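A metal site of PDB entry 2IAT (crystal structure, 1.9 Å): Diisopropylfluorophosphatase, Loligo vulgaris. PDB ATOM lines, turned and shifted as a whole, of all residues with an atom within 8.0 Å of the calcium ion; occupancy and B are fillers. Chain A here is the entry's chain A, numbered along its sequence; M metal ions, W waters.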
ATOM      1  N   GLU A  19      -6.106 -13.360  11.679  1.00  0.00           N
ATOM      2  CA  GLU A  19      -5.027 -14.234  11.259  1.00  0.00           C
ATOM      3  C   GLU A  19      -4.775 -14.207   9.760  1.00  0.00           C
ATOM      4  O   GLU A  19      -5.447 -13.486   9.013  1.00  0.00           O
ATOM      5  CB  GLU A  19      -5.384 -15.672  11.641  1.00  0.00           C
ATOM      6  CG  GLU A  19      -4.652 -16.214  12.848  1.00  0.00           C
ATOM      7  CD  GLU A  19      -3.311 -16.812  12.496  1.00  0.00           C
ATOM      8  OE1 GLU A  19      -2.788 -16.540  11.384  1.00  0.00           O
ATOM      9  OE2 GLU A  19      -2.788 -17.568  13.324  1.00  0.00           O
ATOM     10  N   GLY A  20      -3.818 -15.027   9.347  1.00  0.00           N
ATOM     11  CA  GLY A  20      -3.443 -15.192   7.958  1.00  0.00           C
ATOM     12  C   GLY A  20      -3.321 -13.991   7.023  1.00  0.00           C
ATOM     13  O   GLY A  20      -3.807 -14.073   5.896  1.00  0.00           O
ATOM     14  N   PRO A  21      -2.646 -12.910   7.431  1.00  0.00           N
ATOM     15  CA  PRO A  21      -2.480 -11.713   6.580  1.00  0.00           C
ATOM     16  C   PRO A  21      -1.821 -12.083   5.243  1.00  0.00           C
ATOM     17  O   PRO A  21      -0.833 -12.828   5.205  1.00  0.00           O
ATOM     18  CB  PRO A  21      -1.594 -10.798   7.429  1.00  0.00           C
ATOM     19  CG  PRO A  21      -0.816 -11.763   8.289  1.00  0.00           C
ATOM     20  CD  PRO A  21      -1.860 -12.770   8.678  1.00  0.00           C
ATOM     21  N   VAL A  22      -2.367 -11.562   4.144  1.00  0.00           N
ATOM     22  CA  VAL A  22      -1.817 -11.880   2.832  1.00  0.00           C
ATOM     23  C   VAL A  22      -2.138 -10.849   1.763  1.00  0.00           C
ATOM     24  O   VAL A  22      -3.164 -10.147   1.828  1.00  0.00           O
ATOM     25  CB  VAL A  22      -2.318 -13.284   2.364  1.00  0.00           C
ATOM     26  CG1 VAL A  22      -3.831 -13.247   2.093  1.00  0.00           C
ATOM     27  CG2 VAL A  22      -1.555 -13.741   1.120  1.00  0.00           C
ATOM     28  N   PHE A  23      -1.215 -10.691   0.825  1.00  0.00           N
ATOM     29  CA  PHE A  23      -1.391  -9.783  -0.297  1.00  0.00           C
ATOM     30  C   PHE A  23      -1.482 -10.637  -1.564  1.00  0.00           C
ATOM     31  O   PHE A  23      -0.791 -11.663  -1.679  1.00  0.00           O
ATOM     32  CB  PHE A  23      -0.188  -8.838  -0.424  1.00  0.00           C
ATOM     33  CG  PHE A  23      -0.226  -7.687   0.536  1.00  0.00           C
ATOM     34  CD1 PHE A  23       0.485  -7.725   1.729  1.00  0.00           C
ATOM     35  CD2 PHE A  23      -0.937  -6.531   0.212  1.00  0.00           C
ATOM     36  CE1 PHE A  23       0.492  -6.629   2.586  1.00  0.00           C
ATOM     37  CE2 PHE A  23      -0.942  -5.439   1.062  1.00  0.00           C
ATOM     38  CZ  PHE A  23      -0.223  -5.482   2.259  1.00  0.00           C
ATOM     39  N   CYS A  74      -3.006 -18.097   5.234  1.00  0.00           N
ATOM     40  CA  CYS A  74      -3.081 -17.884   3.796  1.00  0.00           C
ATOM     41  C   CYS A  74      -1.756 -17.810   3.038  1.00  0.00           C
ATOM     42  O   CYS A  74      -0.702 -17.512   3.601  1.00  0.00           O
ATOM     43  CB  CYS A  74      -3.838 -16.593   3.517  1.00  0.00           C
ATOM     44  SG  CYS A  74      -5.461 -16.504   4.280  1.00  0.00           S
ATOM     45  N   GLN A  75      -1.855 -18.044   1.740  1.00  0.00           N
ATOM     46  CA  GLN A  75      -0.756 -17.966   0.786  1.00  0.00           C
ATOM     47  C   GLN A  75      -1.419 -17.637  -0.549  1.00  0.00           C
ATOM     48  O   GLN A  75      -2.488 -18.165  -0.868  1.00  0.00           O
ATOM     49  CB  GLN A  75      -0.001 -19.301   0.641  1.00  0.00           C
ATOM     50  CG  GLN A  75       0.968 -19.625   1.772  1.00  0.00           C
ATOM     51  CD  GLN A  75       2.080 -18.607   1.912  1.00  0.00           C
ATOM     52  OE1 GLN A  75       1.940 -17.591   2.595  1.00  0.00           O
ATOM     53  NE2 GLN A  75       3.214 -18.890   1.280  1.00  0.00           N
ATOM     54  N   ASP A 119      -1.744 -23.050   8.965  1.00  0.00           N
ATOM     55  CA  ASP A 119      -0.939 -22.141   8.164  1.00  0.00           C
ATOM     56  C   ASP A 119      -0.226 -22.920   7.056  1.00  0.00           C
ATOM     57  O   ASP A 119      -0.124 -24.144   7.115  1.00  0.00           O
ATOM     58  CB  ASP A 119       0.077 -21.382   9.027  1.00  0.00           C
ATOM     59  CG  ASP A 119       0.339 -19.952   8.527  1.00  0.00           C
ATOM     60  OD1 ASP A 119      -0.057 -19.619   7.390  1.00  0.00           O
ATOM     61  OD2 ASP A 119       0.930 -19.153   9.281  1.00  0.00           O
ATOM     62  N   CYS A 120       0.236 -22.201   6.048  1.00  0.00           N
ATOM     63  CA  CYS A 120       0.943 -22.810   4.920  1.00  0.00           C
ATOM     64  C   CYS A 120       1.978 -21.881   4.310  1.00  0.00           C
ATOM     65  O   CYS A 120       1.934 -20.658   4.509  1.00  0.00           O
ATOM     66  CB  CYS A 120      -0.051 -23.252   3.845  1.00  0.00           C
ATOM     67  SG  CYS A 120      -1.161 -21.962   3.269  1.00  0.00           S
ATOM     68  N   ILE A 175       4.786 -21.755   9.549  1.00  0.00           N
ATOM     69  CA  ILE A 175       5.647 -22.534   8.672  1.00  0.00           C
ATOM     70  C   ILE A 175       6.216 -21.605   7.614  1.00  0.00           C
ATOM     71  O   ILE A 175       5.547 -20.671   7.180  1.00  0.00           O
ATOM     72  CB  ILE A 175       4.855 -23.731   8.041  1.00  0.00           C
ATOM     73  CG1 ILE A 175       5.779 -24.643   7.237  1.00  0.00           C
ATOM     74  CG2 ILE A 175       3.701 -23.225   7.188  1.00  0.00           C
ATOM     75  CD1 ILE A 175       5.160 -25.973   6.888  1.00  0.00           C
ATOM     76  N   GLY A 228       2.646 -17.219  13.744  1.00  0.00           N
ATOM     77  CA  GLY A 228       2.958 -17.001  12.340  1.00  0.00           C
ATOM     78  C   GLY A 228       4.430 -16.684  12.142  1.00  0.00           C
ATOM     79  O   GLY A 228       5.094 -16.266  13.095  1.00  0.00           O
ATOM     80  N   MET A 229       4.945 -16.854  10.919  1.00  0.00           N
ATOM     81  CA  MET A 229       6.347 -16.565  10.602  1.00  0.00           C
ATOM     82  C   MET A 229       6.587 -16.278   9.120  1.00  0.00           C
ATOM     83  O   MET A 229       5.843 -16.737   8.254  1.00  0.00           O
ATOM     84  CB  MET A 229       7.239 -17.751  11.006  1.00  0.00           C
ATOM     85  CG  MET A 229       7.013 -19.000  10.188  1.00  0.00           C
ATOM     86  SD  MET A 229       8.203 -20.301  10.467  1.00  0.00           S
ATOM     87  CE  MET A 229       8.021 -20.521  12.210  1.00  0.00           C
ATOM     88  N   ASP A 230       7.670 -15.553   8.857  1.00  0.00           N
ATOM     89  CA  ASP A 230       8.081 -15.194   7.492  1.00  0.00           C
ATOM     90  C   ASP A 230       9.536 -14.749   7.472  1.00  0.00           C
ATOM     91  O   ASP A 230      10.084 -14.259   8.464  1.00  0.00           O
ATOM     92  CB  ASP A 230       7.238 -14.048   6.945  1.00  0.00           C
ATOM     93  CG  ASP A 230       6.110 -14.518   6.032  1.00  0.00           C
ATOM     94  OD1 ASP A 230       6.246 -15.529   5.312  1.00  0.00           O
ATOM     95  OD2 ASP A 230       5.084 -13.825   6.036  1.00  0.00           O
ATOM     96  N   PHE A 231      10.130 -14.860   6.285  1.00  0.00           N
ATOM     97  CA  PHE A 231      11.521 -14.474   6.074  1.00  0.00           C
ATOM     98  C   PHE A 231      11.648 -13.081   5.450  1.00  0.00           C
ATOM     99  O   PHE A 231      10.791 -12.676   4.663  1.00  0.00           O
ATOM    100  CB  PHE A 231      12.194 -15.444   5.107  1.00  0.00           C
ATOM    101  CG  PHE A 231      12.615 -16.738   5.726  1.00  0.00           C
ATOM    102  CD1 PHE A 231      11.972 -17.919   5.367  1.00  0.00           C
ATOM    103  CD2 PHE A 231      13.689 -16.792   6.603  1.00  0.00           C
ATOM    104  CE1 PHE A 231      12.395 -19.149   5.881  1.00  0.00           C
ATOM    105  CE2 PHE A 231      14.121 -18.011   7.137  1.00  0.00           C
ATOM    106  CZ  PHE A 231      13.484 -19.190   6.769  1.00  0.00           C
ATOM    107  N   LEU A 238      11.369 -13.810  10.970  1.00  0.00           N
ATOM    108  CA  LEU A 238      10.594 -13.064  11.964  1.00  0.00           C
ATOM    109  C   LEU A 238       9.434 -13.946  12.401  1.00  0.00           C
ATOM    110  O   LEU A 238       8.697 -14.484  11.583  1.00  0.00           O
ATOM    111  CB  LEU A 238      10.113 -11.714  11.402  1.00  0.00           C
ATOM    112  CG  LEU A 238      11.247 -10.691  11.201  1.00  0.00           C
ATOM    113  CD1 LEU A 238      12.112 -11.095  10.016  1.00  0.00           C
ATOM    114  CD2 LEU A 238      10.708  -9.298  10.979  1.00  0.00           C
ATOM    115  N   ASN A 270       0.139 -13.320  13.586  1.00  0.00           N
ATOM    116  CA  ASN A 270       0.747 -13.638  12.310  1.00  0.00           C
ATOM    117  C   ASN A 270       1.230 -12.336  11.671  1.00  0.00           C
ATOM    118  O   ASN A 270       0.910 -11.241  12.154  1.00  0.00           O
ATOM    119  CB  ASN A 270      -0.267 -14.375  11.417  1.00  0.00           C
ATOM    120  CG  ASN A 270       0.387 -15.425  10.495  1.00  0.00           C
ATOM    121  OD1 ASN A 270      -0.169 -16.503  10.254  1.00  0.00           O
ATOM    122  ND2 ASN A 270       1.561 -15.096   9.976  1.00  0.00           N
ATOM    123  N   LEU A 271       2.049 -12.452  10.631  1.00  0.00           N
ATOM    124  CA  LEU A 271       2.557 -11.277   9.948  1.00  0.00           C
ATOM    125  C   LEU A 271       2.731 -11.547   8.465  1.00  0.00           C
ATOM    126  O   LEU A 271       2.618 -12.691   8.043  1.00  0.00           O
ATOM    127  CB  LEU A 271       3.886 -10.812  10.579  1.00  0.00           C
ATOM    128  CG  LEU A 271       4.981 -11.837  10.911  1.00  0.00           C
ATOM    129  CD1 LEU A 271       5.770 -12.211   9.662  1.00  0.00           C
ATOM    130  CD2 LEU A 271       5.909 -11.247  11.960  1.00  0.00           C
ATOM    131  N   HIS A 272       2.941 -10.498   7.686  1.00  0.00           N
ATOM    132  CA  HIS A 272       3.136 -10.631   6.240  1.00  0.00           C
ATOM    133  C   HIS A 272       3.684  -9.302   5.729  1.00  0.00           C
ATOM    134  O   HIS A 272       3.259  -8.231   6.168  1.00  0.00           O
ATOM    135  CB  HIS A 272       1.799 -10.966   5.547  1.00  0.00           C
ATOM    136  CG  HIS A 272       1.967 -11.721   4.254  1.00  0.00           C
ATOM    137  ND1 HIS A 272       2.171 -13.077   4.209  1.00  0.00           N
ATOM    138  CD2 HIS A 272       1.960 -11.298   2.967  1.00  0.00           C
ATOM    139  CE1 HIS A 272       2.286 -13.459   2.942  1.00  0.00           C
ATOM    140  NE2 HIS A 272       2.160 -12.394   2.174  1.00  0.00           N
ATOM    141  N   PHE A 273       4.679  -9.387   4.848  1.00  0.00           N
ATOM    142  CA  PHE A 273       5.280  -8.184   4.263  1.00  0.00           C
ATOM    143  C   PHE A 273       4.438  -7.688   3.099  1.00  0.00           C
ATOM    144  O   PHE A 273       3.746  -8.467   2.442  1.00  0.00           O
ATOM    145  CB  PHE A 273       6.678  -8.490   3.704  1.00  0.00           C
ATOM    146  CG  PHE A 273       7.756  -8.568   4.745  1.00  0.00           C
ATOM    147  CD1 PHE A 273       7.976  -9.728   5.468  1.00  0.00           C
ATOM    148  CD2 PHE A 273       8.609  -7.482   4.953  1.00  0.00           C
ATOM    149  CE1 PHE A 273       9.030  -9.826   6.385  1.00  0.00           C
ATOM    150  CE2 PHE A 273       9.666  -7.571   5.873  1.00  0.00           C
ATOM    151  CZ  PHE A 273       9.868  -8.753   6.582  1.00  0.00           C
ATOM    152  N   ILE A 280       5.573  -4.508   7.406  1.00  0.00           N
ATOM    153  CA  ILE A 280       5.080  -5.789   7.888  1.00  0.00           C
ATOM    154  C   ILE A 280       3.730  -5.597   8.573  1.00  0.00           C
ATOM    155  O   ILE A 280       3.643  -4.905   9.584  1.00  0.00           O
ATOM    156  CB  ILE A 280       6.035  -6.414   8.930  1.00  0.00           C
ATOM    157  CG1 ILE A 280       7.424  -6.596   8.353  1.00  0.00           C
ATOM    158  CG2 ILE A 280       5.463  -7.753   9.402  1.00  0.00           C
ATOM    159  CD1 ILE A 280       8.403  -7.229   9.338  1.00  0.00           C
ATOM    160  N   PHE A 281       2.699  -6.201   8.015  1.00  0.00           N
ATOM    161  CA  PHE A 281       1.361  -6.143   8.600  1.00  0.00           C
ATOM    162  C   PHE A 281       1.292  -7.254   9.655  1.00  0.00           C
ATOM    163  O   PHE A 281       1.728  -8.375   9.415  1.00  0.00           O
ATOM    164  CB  PHE A 281       0.286  -6.306   7.528  1.00  0.00           C
ATOM    165  CG  PHE A 281       0.115  -5.080   6.657  1.00  0.00           C
ATOM    166  CD1 PHE A 281      -1.005  -4.274   6.803  1.00  0.00           C
ATOM    167  CD2 PHE A 281       1.099  -4.712   5.735  1.00  0.00           C
ATOM    168  CE1 PHE A 281      -1.162  -3.107   6.036  1.00  0.00           C
ATOM    169  CE2 PHE A 281       0.960  -3.561   4.965  1.00  0.00           C
ATOM    170  CZ  PHE A 281      -0.173  -2.752   5.115  1.00  0.00           C
ATOM    171  N   GLN A 302       7.395 -13.692  -1.867  1.00  0.00           N
ATOM    172  CA  GLN A 302       6.507 -14.847  -1.731  1.00  0.00           C
ATOM    173  C   GLN A 302       6.437 -15.516  -3.104  1.00  0.00           C
ATOM    174  O   GLN A 302       6.876 -14.940  -4.105  1.00  0.00           O
ATOM    175  CB  GLN A 302       5.109 -14.386  -1.297  1.00  0.00           C
ATOM    176  CG  GLN A 302       5.002 -13.965   0.173  1.00  0.00           C
ATOM    177  CD  GLN A 302       4.938 -15.137   1.124  1.00  0.00           C
ATOM    178  OE1 GLN A 302       5.911 -15.474   1.805  1.00  0.00           O
ATOM    179  NE2 GLN A 302       3.776 -15.776   1.190  1.00  0.00           N
HETATM  180 CA    CA M   1       2.773 -14.334   6.365  1.00  0.00          CA
HETATM  181  O   HOH W   1       3.542 -16.249   4.807  1.00  0.00           O
HETATM  182  O   HOH W   2       0.294 -14.551   6.635  1.00  0.00           O
HETATM  183  O   HOH W   3       3.216 -16.103   8.106  1.00  0.00           O
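A ring nitrogen (ND1) of His 272 lies close to the backbone carbonyl oxygen of Pro 21 (3.2 Å).
OD1 of Asn 270 sits close to OD2 of Asp 119, at 3.0 Å.
N of Phe 281 sits at hydrogen-bond distance from O of His 272, at 2.8 Å.
The backbone NH (N) of Leu 238 lies within hydrogen-bond range of the backbone carbonyl oxygen (O) of Asp 230 (2.9 Å).
The side-chain amide oxygen (OD1) of Asn 270 lies close to the side-chain carboxylate (OE1) of Glu 19, 2.9 Å away.
ND2 of Asn 270 touches the calcium ion, at 3.9 Å.
The calcium ion is bound by O of Leu 271 (2.4 Å), OD2 of Asp 230 (2.4 Å), water W2 (2.5 Å), water W3 (2.5 Å), ND1 of His 272 (2.6 Å) and water W1 (2.6 Å).
Water W1 lies within hydrogen-bond range of the side-chain carboxylate (OD1) of Asp 230 (2.8 Å) and the side-chain amide oxygen (OE1) of Gln 75 (3.0 Å).
Water W3 bridges ND2 of Asn 270 and O of Met 229.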
